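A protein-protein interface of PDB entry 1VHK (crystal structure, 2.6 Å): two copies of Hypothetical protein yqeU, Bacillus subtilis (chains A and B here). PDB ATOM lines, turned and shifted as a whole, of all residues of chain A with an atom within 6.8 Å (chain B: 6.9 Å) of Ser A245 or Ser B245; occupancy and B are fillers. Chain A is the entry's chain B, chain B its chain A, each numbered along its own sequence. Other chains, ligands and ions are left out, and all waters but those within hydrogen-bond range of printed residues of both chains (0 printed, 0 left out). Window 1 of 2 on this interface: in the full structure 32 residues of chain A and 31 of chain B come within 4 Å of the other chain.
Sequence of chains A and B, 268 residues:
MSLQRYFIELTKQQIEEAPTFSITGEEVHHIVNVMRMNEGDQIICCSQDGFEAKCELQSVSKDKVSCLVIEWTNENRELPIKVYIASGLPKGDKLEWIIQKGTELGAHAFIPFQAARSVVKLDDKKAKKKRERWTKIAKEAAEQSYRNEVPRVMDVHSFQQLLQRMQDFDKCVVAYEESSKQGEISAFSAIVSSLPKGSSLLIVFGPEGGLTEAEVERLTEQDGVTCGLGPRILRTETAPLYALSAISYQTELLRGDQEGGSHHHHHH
The side-chain hydroxyl (OG) of Ser B248 sits at hydrogen-bond distance from the guanidinium group (NH1) of Arg A232 (3.4 Å). The guanidinium group (NH1) of Arg A232 lies within salt-bridge range of the side-chain carboxylate (OE2) of Glu B252, 2.9 Å away. The side-chain hydroxyl of Ser B248 is in hydrogen-bond range of the side-chain hydroxyl of Tyr A242, 2.6 Å away. The side-chain amide oxygen (OE1) of Gln A250 lies within hydrogen-bond range of the side-chain hydroxyl (OH) of Tyr B249 (2.4 Å). NE2 of Gln B250 sits at hydrogen-bond distance from OH of Tyr A249 (2.5 Å). OH of Tyr B242 sits at hydrogen-bond distance from OG of Ser A248 (2.5 Å).
O of Ser B248 sits at hydrogen-bond distance from N of Leu B253, 3.4 Å away. O of Leu A241 sits at hydrogen-bond distance from OG of Ser A245, at 3.0 Å. The side-chain hydroxyl of Ser B248 sits at hydrogen-bond distance from the side-chain carboxylate of Glu B252. The backbone NH (N) of Leu A253 is in hydrogen-bond range of the backbone carbonyl oxygen (O) of Ser A248. OG of Ser B245 lies within hydrogen-bond range of O of Leu B241.
Leu A105 touches Tyr B242 (CD2 to CD1, 3.7 Å). Arg A232 touches Leu B105 (NE to C, 3.5 Å). CD2 of Leu B105 touches CD1 of Tyr A242, 3.5 Å away. N of Tyr B249 touches OH of Tyr A242, 3.7 Å away. OG of Ser A245 touches CA of Tyr B242 (3.0 Å). Tyr B249 touches Ala A246. Tyr B242 touches Tyr A249 (OH to N, 3.9 Å). CB of Ala B246 touches CD1 of Tyr A249, at 3.7 Å. Tyr A249 touches Tyr B249. CD1 of Leu A253 touches OH of Tyr B242, 3.7 Å away.
Printed residues of chain B within 4 Å of Leu A105: Tyr B242. Ser A245 touches just these residues of chain B: Tyr B242 (3.0 Å) and Ser B245 (3.6 Å). Ser B245 touches just these residues of chain A: Tyr A242 and Ser A245. Of the printed residues of chain A, Tyr B249 touches Tyr A242 (3.7 Å), Ala A246 (3.6 Å), Tyr A249 (3.4 Å) and Gln A250 (2.4 Å). Of the printed residues of chain A, Leu B253 touches Tyr A242 (3.7 Å). The nearest residue of chain B that does not touch Ser A245 is Leu B241 (4.4 Å).
Printed residues of chain A that touch a printed residue of chain B: Leu A105, Arg A232, Tyr A242, Ser A245, Ala A246, Ser A248, Tyr A249, Gln A250 and Leu A253. Of the 16 printed residues of chain B, 9 touch a printed residue of chain A. Hydrophobic or aromatic side chains of chain B within 4 Å of the printed part of chain A: Leu B105, Tyr B242, Ala B246, Tyr B249 and Leu B253. Among the printed residues, Asp or Glu carboxylates within 4 Å of a Lys or Arg side-chain nitrogen of the other chain: Arg A232 with Glu B252 (2.9 Å).
Tyr A242 touches Ser B248, and with the chains exchanged Ser A248 touches Tyr B242. Tyr A242 touches Leu B253, and with the chains exchanged Leu A253 touches Tyr B242. Ala A246 touches Tyr B249, and with the chains exchanged Tyr A249 touches Ala B246. Tyr A249 touches Gln B250, and with the chains exchanged Gln A250 touches Tyr B249. Positions printed for both chains: 105, 238, 240, 241, 242, 243, 244, 245, 246, 247, 248, 249, 250 and 253. Of the 19 pairs that touch across the chains among the printed residues, 16 have their exchanged pair printed and touching as well.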
ATOM      1  N   LEU A 105      11.587 -23.726 -14.616  1.00  0.00           N
ATOM      2  CA  LEU A 105      12.712 -24.537 -14.946  1.00  0.00           C
ATOM      3  C   LEU A 105      12.373 -25.967 -15.327  1.00  0.00           C
ATOM      4  O   LEU A 105      13.298 -26.804 -15.366  1.00  0.00           O
ATOM      5  CB  LEU A 105      13.741 -24.521 -13.807  1.00  0.00           C
ATOM      6  CG  LEU A 105      14.475 -23.231 -13.526  1.00  0.00           C
ATOM      7  CD1 LEU A 105      15.208 -23.269 -12.182  1.00  0.00           C
ATOM      8  CD2 LEU A 105      15.502 -22.903 -14.612  1.00  0.00           C
ATOM      9  N   ARG A 232      29.664 -26.708  -3.654  1.00  0.00           N
ATOM     10  CA  ARG A 232      29.277 -25.568  -2.783  1.00  0.00           C
ATOM     11  C   ARG A 232      28.027 -25.861  -1.983  1.00  0.00           C
ATOM     12  O   ARG A 232      27.068 -26.504  -2.428  1.00  0.00           O
ATOM     13  CB  ARG A 232      29.155 -24.266  -3.589  1.00  0.00           C
ATOM     14  CG  ARG A 232      30.463 -23.884  -4.297  1.00  0.00           C
ATOM     15  CD  ARG A 232      30.193 -22.764  -5.349  1.00  0.00           C
ATOM     16  NE  ARG A 232      29.655 -23.381  -6.559  1.00  0.00           N
ATOM     17  CZ  ARG A 232      30.312 -24.232  -7.346  1.00  0.00           C
ATOM     18  NH1 ARG A 232      29.680 -24.766  -8.394  1.00  0.00           N
ATOM     19  NH2 ARG A 232      31.583 -24.522  -7.162  1.00  0.00           N
ATOM     20  N   LEU A 234      24.609 -25.387  -0.968  1.00  0.00           N
ATOM     21  CA  LEU A 234      23.399 -24.783  -1.472  1.00  0.00           C
ATOM     22  C   LEU A 234      22.322 -24.600  -0.418  1.00  0.00           C
ATOM     23  O   LEU A 234      22.034 -25.484   0.397  1.00  0.00           O
ATOM     24  CB  LEU A 234      22.887 -25.700  -2.612  1.00  0.00           C
ATOM     25  CG  LEU A 234      23.371 -25.391  -4.037  1.00  0.00           C
ATOM     26  CD1 LEU A 234      24.776 -24.868  -4.117  1.00  0.00           C
ATOM     27  CD2 LEU A 234      23.236 -26.610  -4.959  1.00  0.00           C
ATOM     28  N   THR A 238      17.781 -23.129  -3.091  1.00  0.00           N
ATOM     29  CA  THR A 238      18.662 -23.087  -4.258  1.00  0.00           C
ATOM     30  C   THR A 238      18.845 -24.462  -4.883  1.00  0.00           C
ATOM     31  O   THR A 238      18.679 -24.616  -6.111  1.00  0.00           O
ATOM     32  CB  THR A 238      20.048 -22.511  -3.886  1.00  0.00           C
ATOM     33  OG1 THR A 238      19.879 -21.320  -3.079  1.00  0.00           O
ATOM     34  CG2 THR A 238      20.865 -22.179  -5.108  1.00  0.00           C
ATOM     35  N   PRO A 240      16.955 -27.301  -5.601  1.00  0.00           N
ATOM     36  CA  PRO A 240      16.092 -27.736  -6.664  1.00  0.00           C
ATOM     37  C   PRO A 240      16.323 -26.949  -7.941  1.00  0.00           C
ATOM     38  O   PRO A 240      16.256 -27.523  -9.044  1.00  0.00           O
ATOM     39  CB  PRO A 240      14.672 -27.482  -6.132  1.00  0.00           C
ATOM     40  CG  PRO A 240      14.812 -27.288  -4.675  1.00  0.00           C
ATOM     41  CD  PRO A 240      16.193 -26.711  -4.472  1.00  0.00           C
ATOM     42  N   LEU A 241      16.685 -25.666  -7.845  1.00  0.00           N
ATOM     43  CA  LEU A 241      16.866 -24.909  -9.081  1.00  0.00           C
ATOM     44  C   LEU A 241      18.117 -25.379  -9.815  1.00  0.00           C
ATOM     45  O   LEU A 241      18.193 -25.293 -11.042  1.00  0.00           O
ATOM     46  CB  LEU A 241      16.898 -23.402  -8.822  1.00  0.00           C
ATOM     47  CG  LEU A 241      15.932 -22.894  -7.754  1.00  0.00           C
ATOM     48  CD1 LEU A 241      15.885 -21.371  -7.763  1.00  0.00           C
ATOM     49  CD2 LEU A 241      14.529 -23.482  -7.909  1.00  0.00           C
ATOM     50  N   TYR A 242      19.142 -25.779  -9.087  1.00  0.00           N
ATOM     51  CA  TYR A 242      20.376 -26.289  -9.662  1.00  0.00           C
ATOM     52  C   TYR A 242      20.098 -27.620 -10.378  1.00  0.00           C
ATOM     53  O   TYR A 242      20.481 -27.795 -11.534  1.00  0.00           O
ATOM     54  CB  TYR A 242      21.403 -26.468  -8.540  1.00  0.00           C
ATOM     55  CG  TYR A 242      22.697 -27.093  -8.989  1.00  0.00           C
ATOM     56  CD1 TYR A 242      23.822 -26.286  -9.177  1.00  0.00           C
ATOM     57  CD2 TYR A 242      22.809 -28.464  -9.238  1.00  0.00           C
ATOM     58  CE1 TYR A 242      25.004 -26.831  -9.604  1.00  0.00           C
ATOM     59  CE2 TYR A 242      24.002 -29.005  -9.679  1.00  0.00           C
ATOM     60  CZ  TYR A 242      25.092 -28.178  -9.856  1.00  0.00           C
ATOM     61  OH  TYR A 242      26.298 -28.700 -10.284  1.00  0.00           O
ATOM     62  N   ALA A 243      19.415 -28.546  -9.663  1.00  0.00           N
ATOM     63  CA  ALA A 243      19.149 -29.851 -10.229  1.00  0.00           C
ATOM     64  C   ALA A 243      18.398 -29.728 -11.554  1.00  0.00           C
ATOM     65  O   ALA A 243      18.781 -30.333 -12.544  1.00  0.00           O
ATOM     66  CB  ALA A 243      18.397 -30.755  -9.250  1.00  0.00           C
ATOM     67  N   LEU A 244      17.304 -28.974 -11.570  1.00  0.00           N
ATOM     68  CA  LEU A 244      16.504 -28.730 -12.738  1.00  0.00           C
ATOM     69  C   LEU A 244      17.316 -28.078 -13.871  1.00  0.00           C
ATOM     70  O   LEU A 244      17.062 -28.324 -15.060  1.00  0.00           O
ATOM     71  CB  LEU A 244      15.318 -27.809 -12.375  1.00  0.00           C
ATOM     72  CG  LEU A 244      14.215 -28.443 -11.545  1.00  0.00           C
ATOM     73  CD1 LEU A 244      13.265 -27.419 -10.954  1.00  0.00           C
ATOM     74  CD2 LEU A 244      13.458 -29.469 -12.395  1.00  0.00           C
ATOM     75  N   SER A 245      18.192 -27.137 -13.513  1.00  0.00           N
ATOM     76  CA  SER A 245      18.984 -26.456 -14.525  1.00  0.00           C
ATOM     77  C   SER A 245      19.968 -27.437 -15.180  1.00  0.00           C
ATOM     78  O   SER A 245      20.259 -27.341 -16.362  1.00  0.00           O
ATOM     79  CB  SER A 245      19.783 -25.287 -13.929  1.00  0.00           C
ATOM     80  OG  SER A 245      18.974 -24.178 -13.700  1.00  0.00           O
ATOM     81  N   ALA A 246      20.618 -28.206 -14.308  1.00  0.00           N
ATOM     82  CA  ALA A 246      21.576 -29.215 -14.742  1.00  0.00           C
ATOM     83  C   ALA A 246      20.838 -30.194 -15.660  1.00  0.00           C
ATOM     84  O   ALA A 246      21.257 -30.440 -16.780  1.00  0.00           O
ATOM     85  CB  ALA A 246      22.157 -29.939 -13.551  1.00  0.00           C
ATOM     86  N   ILE A 247      19.620 -30.577 -15.250  1.00  0.00           N
ATOM     87  CA  ILE A 247      18.846 -31.492 -16.091  1.00  0.00           C
ATOM     88  C   ILE A 247      18.550 -30.966 -17.468  1.00  0.00           C
ATOM     89  O   ILE A 247      18.734 -31.718 -18.445  1.00  0.00           O
ATOM     90  CB  ILE A 247      17.632 -32.032 -15.371  1.00  0.00           C
ATOM     91  CG1 ILE A 247      18.116 -33.034 -14.283  1.00  0.00           C
ATOM     92  CG2 ILE A 247      16.679 -32.731 -16.319  1.00  0.00           C
ATOM     93  CD1 ILE A 247      17.062 -33.242 -13.203  1.00  0.00           C
ATOM     94  N   SER A 248      18.128 -29.739 -17.630  1.00  0.00           N
ATOM     95  CA  SER A 248      17.856 -29.109 -18.906  1.00  0.00           C
ATOM     96  C   SER A 248      19.150 -29.038 -19.732  1.00  0.00           C
ATOM     97  O   SER A 248      19.174 -29.297 -20.937  1.00  0.00           O
ATOM     98  CB  SER A 248      17.281 -27.723 -18.707  1.00  0.00           C
ATOM     99  OG  SER A 248      17.451 -26.923 -19.888  1.00  0.00           O
ATOM    100  N   TYR A 249      20.264 -28.748 -19.010  1.00  0.00           N
ATOM    101  CA  TYR A 249      21.550 -28.681 -19.678  1.00  0.00           C
ATOM    102  C   TYR A 249      21.904 -30.013 -20.358  1.00  0.00           C
ATOM    103  O   TYR A 249      22.142 -30.018 -21.572  1.00  0.00           O
ATOM    104  CB  TYR A 249      22.634 -28.197 -18.739  1.00  0.00           C
ATOM    105  CG  TYR A 249      23.975 -28.016 -19.415  1.00  0.00           C
ATOM    106  CD1 TYR A 249      24.227 -26.968 -20.268  1.00  0.00           C
ATOM    107  CD2 TYR A 249      24.978 -28.956 -19.213  1.00  0.00           C
ATOM    108  CE1 TYR A 249      25.468 -26.815 -20.879  1.00  0.00           C
ATOM    109  CE2 TYR A 249      26.209 -28.841 -19.853  1.00  0.00           C
ATOM    110  CZ  TYR A 249      26.436 -27.759 -20.670  1.00  0.00           C
ATOM    111  OH  TYR A 249      27.679 -27.622 -21.263  1.00  0.00           O
ATOM    112  N   GLN A 250      21.917 -31.118 -19.666  1.00  0.00           N
ATOM    113  CA  GLN A 250      22.158 -32.441 -20.124  1.00  0.00           C
ATOM    114  C   GLN A 250      21.216 -32.905 -21.239  1.00  0.00           C
ATOM    115  O   GLN A 250      21.674 -33.262 -22.334  1.00  0.00           O
ATOM    116  CB  GLN A 250      22.015 -33.431 -18.933  1.00  0.00           C
ATOM    117  CG  GLN A 250      22.304 -34.886 -19.290  1.00  0.00           C
ATOM    118  CD  GLN A 250      23.686 -35.043 -19.893  1.00  0.00           C
ATOM    119  OE1 GLN A 250      24.678 -34.608 -19.316  1.00  0.00           O
ATOM    120  NE2 GLN A 250      23.765 -35.583 -21.102  1.00  0.00           N
ATOM    121  N   LEU A 253      20.457 -29.078 -23.925  1.00  0.00           N
ATOM    122  CA  LEU A 253      21.459 -28.237 -24.604  1.00  0.00           C
ATOM    123  C   LEU A 253      22.593 -29.094 -25.164  1.00  0.00           C
ATOM    124  O   LEU A 253      23.273 -28.714 -26.129  1.00  0.00           O
ATOM    125  CB  LEU A 253      21.983 -27.146 -23.724  1.00  0.00           C
ATOM    126  CG  LEU A 253      21.114 -26.068 -23.106  1.00  0.00           C
ATOM    127  CD1 LEU A 253      22.006 -25.067 -22.334  1.00  0.00           C
ATOM    128  CD2 LEU A 253      20.271 -25.335 -24.122  1.00  0.00           C
ATOM    129  N   LEU B 105      25.937 -20.317  -6.109  1.00  0.00           N
ATOM    130  CA  LEU B 105      26.300 -21.017  -7.286  1.00  0.00           C
ATOM    131  C   LEU B 105      27.664 -20.803  -7.899  1.00  0.00           C
ATOM    132  O   LEU B 105      27.905 -21.317  -9.019  1.00  0.00           O
ATOM    133  CB  LEU B 105      25.201 -20.887  -8.368  1.00  0.00           C
ATOM    134  CG  LEU B 105      23.861 -21.475  -7.909  1.00  0.00           C
ATOM    135  CD1 LEU B 105      22.714 -20.863  -8.687  1.00  0.00           C
ATOM    136  CD2 LEU B 105      23.859 -23.000  -7.998  1.00  0.00           C
ATOM    137  N   THR B 238      16.031 -15.548 -12.520  1.00  0.00           N
ATOM    138  CA  THR B 238      16.154 -16.972 -12.801  1.00  0.00           C
ATOM    139  C   THR B 238      17.227 -17.330 -13.806  1.00  0.00           C
ATOM    140  O   THR B 238      18.047 -18.235 -13.524  1.00  0.00           O
ATOM    141  CB  THR B 238      14.819 -17.605 -13.236  1.00  0.00           C
ATOM    142  OG1 THR B 238      13.744 -17.097 -12.428  1.00  0.00           O
ATOM    143  CG2 THR B 238      14.849 -19.117 -13.085  1.00  0.00           C
ATOM    144  N   ALA B 239      17.378 -16.604 -14.893  1.00  0.00           N
ATOM    145  CA  ALA B 239      18.340 -16.842 -15.951  1.00  0.00           C
ATOM    146  C   ALA B 239      19.767 -17.091 -15.523  1.00  0.00           C
ATOM    147  O   ALA B 239      20.383 -18.076 -15.938  1.00  0.00           O
ATOM    148  CB  ALA B 239      18.330 -15.708 -16.980  1.00  0.00           C
ATOM    149  N   PRO B 240      20.370 -16.221 -14.724  1.00  0.00           N
ATOM    150  CA  PRO B 240      21.725 -16.389 -14.253  1.00  0.00           C
ATOM    151  C   PRO B 240      21.930 -17.616 -13.360  1.00  0.00           C
ATOM    152  O   PRO B 240      23.050 -18.129 -13.241  1.00  0.00           O
ATOM    153  CB  PRO B 240      22.030 -15.143 -13.465  1.00  0.00           C
ATOM    154  CG  PRO B 240      20.895 -14.239 -13.593  1.00  0.00           C
ATOM    155  CD  PRO B 240      19.780 -14.945 -14.292  1.00  0.00           C
ATOM    156  N   LEU B 241      20.883 -18.035 -12.678  1.00  0.00           N
ATOM    157  CA  LEU B 241      20.936 -19.185 -11.785  1.00  0.00           C
ATOM    158  C   LEU B 241      21.081 -20.479 -12.598  1.00  0.00           C
ATOM    159  O   LEU B 241      22.000 -21.247 -12.356  1.00  0.00           O
ATOM    160  CB  LEU B 241      19.662 -19.226 -10.950  1.00  0.00           C
ATOM    161  CG  LEU B 241      19.694 -18.505  -9.606  1.00  0.00           C
ATOM    162  CD1 LEU B 241      20.604 -17.267  -9.601  1.00  0.00           C
ATOM    163  CD2 LEU B 241      18.274 -18.135  -9.220  1.00  0.00           C
ATOM    164  N   TYR B 242      20.235 -20.604 -13.614  1.00  0.00           N
ATOM    165  CA  TYR B 242      20.351 -21.680 -14.593  1.00  0.00           C
ATOM    166  C   TYR B 242      21.763 -21.707 -15.182  1.00  0.00           C
ATOM    167  O   TYR B 242      22.463 -22.729 -15.232  1.00  0.00           O
ATOM    168  CB  TYR B 242      19.342 -21.388 -15.717  1.00  0.00           C
ATOM    169  CG  TYR B 242      19.331 -22.357 -16.859  1.00  0.00           C
ATOM    170  CD1 TYR B 242      18.306 -23.294 -16.946  1.00  0.00           C
ATOM    171  CD2 TYR B 242      20.313 -22.354 -17.855  1.00  0.00           C
ATOM    172  CE1 TYR B 242      18.257 -24.208 -17.984  1.00  0.00           C
ATOM    173  CE2 TYR B 242      20.283 -23.270 -18.885  1.00  0.00           C
ATOM    174  CZ  TYR B 242      19.251 -24.189 -18.951  1.00  0.00           C
ATOM    175  OH  TYR B 242      19.184 -25.111 -19.974  1.00  0.00           O
ATOM    176  N   ALA B 243      22.175 -20.531 -15.703  1.00  0.00           N
ATOM    177  CA  ALA B 243      23.507 -20.432 -16.273  1.00  0.00           C
ATOM    178  C   ALA B 243      24.604 -20.873 -15.321  1.00  0.00           C
ATOM    179  O   ALA B 243      25.516 -21.580 -15.755  1.00  0.00           O
ATOM    180  CB  ALA B 243      23.805 -19.011 -16.757  1.00  0.00           C
ATOM    181  N   LEU B 244      24.605 -20.461 -14.048  1.00  0.00           N
ATOM    182  CA  LEU B 244      25.746 -20.836 -13.206  1.00  0.00           C
ATOM    183  C   LEU B 244      25.664 -22.350 -12.921  1.00  0.00           C
ATOM    184  O   LEU B 244      26.690 -23.003 -12.835  1.00  0.00           O
ATOM    185  CB  LEU B 244      25.866 -20.099 -11.938  1.00  0.00           C
ATOM    186  CG  LEU B 244      26.536 -18.801 -11.652  1.00  0.00           C
ATOM    187  CD1 LEU B 244      27.554 -18.396 -12.684  1.00  0.00           C
ATOM    188  CD2 LEU B 244      25.523 -17.688 -11.347  1.00  0.00           C
ATOM    189  N   SER B 245      24.451 -22.826 -12.700  1.00  0.00           N
ATOM    190  CA  SER B 245      24.197 -24.209 -12.405  1.00  0.00           C
ATOM    191  C   SER B 245      24.611 -25.103 -13.560  1.00  0.00           C
ATOM    192  O   SER B 245      25.325 -26.083 -13.312  1.00  0.00           O
ATOM    193  CB  SER B 245      22.714 -24.445 -12.035  1.00  0.00           C
ATOM    194  OG  SER B 245      22.404 -23.664 -10.877  1.00  0.00           O
ATOM    195  N   ALA B 246      24.330 -24.721 -14.788  1.00  0.00           N
ATOM    196  CA  ALA B 246      24.786 -25.482 -15.957  1.00  0.00           C
ATOM    197  C   ALA B 246      26.306 -25.480 -16.024  1.00  0.00           C
ATOM    198  O   ALA B 246      26.919 -26.543 -16.197  1.00  0.00           O
ATOM    199  CB  ALA B 246      24.161 -24.911 -17.222  1.00  0.00           C
ATOM    200  N   ILE B 247      26.965 -24.340 -15.796  1.00  0.00           N
ATOM    201  CA  ILE B 247      28.445 -24.336 -15.866  1.00  0.00           C
ATOM    202  C   ILE B 247      29.024 -25.315 -14.863  1.00  0.00           C
ATOM    203  O   ILE B 247      29.981 -26.072 -15.123  1.00  0.00           O
ATOM    204  CB  ILE B 247      28.978 -22.903 -15.743  1.00  0.00           C
ATOM    205  CG1 ILE B 247      28.803 -22.159 -17.051  1.00  0.00           C
ATOM    206  CG2 ILE B 247      30.447 -22.837 -15.328  1.00  0.00           C
ATOM    207  CD1 ILE B 247      28.435 -20.698 -16.956  1.00  0.00           C
ATOM    208  N   SER B 248      28.441 -25.335 -13.656  1.00  0.00           N
ATOM    209  CA  SER B 248      28.862 -26.248 -12.615  1.00  0.00           C
ATOM    210  C   SER B 248      28.687 -27.709 -13.040  1.00  0.00           C
ATOM    211  O   SER B 248      29.605 -28.527 -12.860  1.00  0.00           O
ATOM    212  CB  SER B 248      28.113 -26.017 -11.314  1.00  0.00           C
ATOM    213  OG  SER B 248      28.298 -27.096 -10.404  1.00  0.00           O
ATOM    214  N   TYR B 249      27.556 -27.985 -13.695  1.00  0.00           N
ATOM    215  CA  TYR B 249      27.278 -29.351 -14.128  1.00  0.00           C
ATOM    216  C   TYR B 249      28.309 -29.831 -15.134  1.00  0.00           C
ATOM    217  O   TYR B 249      28.835 -30.943 -15.057  1.00  0.00           O
ATOM    218  CB  TYR B 249      25.866 -29.418 -14.685  1.00  0.00           C
ATOM    219  CG  TYR B 249      25.522 -30.789 -15.237  1.00  0.00           C
ATOM    220  CD1 TYR B 249      25.136 -31.842 -14.418  1.00  0.00           C
ATOM    221  CD2 TYR B 249      25.659 -31.010 -16.604  1.00  0.00           C
ATOM    222  CE1 TYR B 249      24.862 -33.083 -14.939  1.00  0.00           C
ATOM    223  CE2 TYR B 249      25.387 -32.241 -17.135  1.00  0.00           C
ATOM    224  CZ  TYR B 249      24.975 -33.272 -16.308  1.00  0.00           C
ATOM    225  OH  TYR B 249      24.675 -34.478 -16.903  1.00  0.00           O
ATOM    226  N   GLN B 250      28.623 -28.974 -16.100  1.00  0.00           N
ATOM    227  CA  GLN B 250      29.573 -29.234 -17.144  1.00  0.00           C
ATOM    228  C   GLN B 250      31.019 -29.292 -16.684  1.00  0.00           C
ATOM    229  O   GLN B 250      31.784 -30.187 -17.078  1.00  0.00           O
ATOM    230  CB  GLN B 250      29.448 -28.145 -18.240  1.00  0.00           C
ATOM    231  CG  GLN B 250      30.599 -28.244 -19.246  1.00  0.00           C
ATOM    232  CD  GLN B 250      30.366 -29.376 -20.237  1.00  0.00           C
ATOM    233  OE1 GLN B 250      31.278 -30.107 -20.578  1.00  0.00           O
ATOM    234  NE2 GLN B 250      29.148 -29.520 -20.738  1.00  0.00           N
ATOM    235  N   GLU B 252      32.187 -29.377 -13.466  1.00  0.00           N
ATOM    236  CA  GLU B 252      32.453 -30.119 -12.258  1.00  0.00           C
ATOM    237  C   GLU B 252      31.785 -31.481 -12.122  1.00  0.00           C
ATOM    238  O   GLU B 252      32.281 -32.318 -11.344  1.00  0.00           O
ATOM    239  CB  GLU B 252      32.076 -29.288 -11.019  1.00  0.00           C
ATOM    240  CG  GLU B 252      32.495 -27.839 -11.045  1.00  0.00           C
ATOM    241  CD  GLU B 252      31.907 -27.061  -9.887  1.00  0.00           C
ATOM    242  OE1 GLU B 252      32.698 -26.410  -9.160  1.00  0.00           O
ATOM    243  OE2 GLU B 252      30.678 -27.129  -9.676  1.00  0.00           O
ATOM    244  N   LEU B 253      30.627 -31.740 -12.680  1.00  0.00           N
ATOM    245  CA  LEU B 253      29.894 -32.970 -12.596  1.00  0.00           C
ATOM    246  C   LEU B 253      30.190 -33.954 -13.710  1.00  0.00           C
ATOM    247  O   LEU B 253      30.064 -35.181 -13.524  1.00  0.00           O
ATOM    248  CB  LEU B 253      28.374 -32.700 -12.507  1.00  0.00           C
ATOM    249  CG  LEU B 253      27.779 -32.851 -11.094  1.00  0.00           C
ATOM    250  CD1 LEU B 253      28.649 -32.125 -10.076  1.00  0.00           C
ATOM    251  CD2 LEU B 253      26.349 -32.352 -11.013  1.00  0.00           C
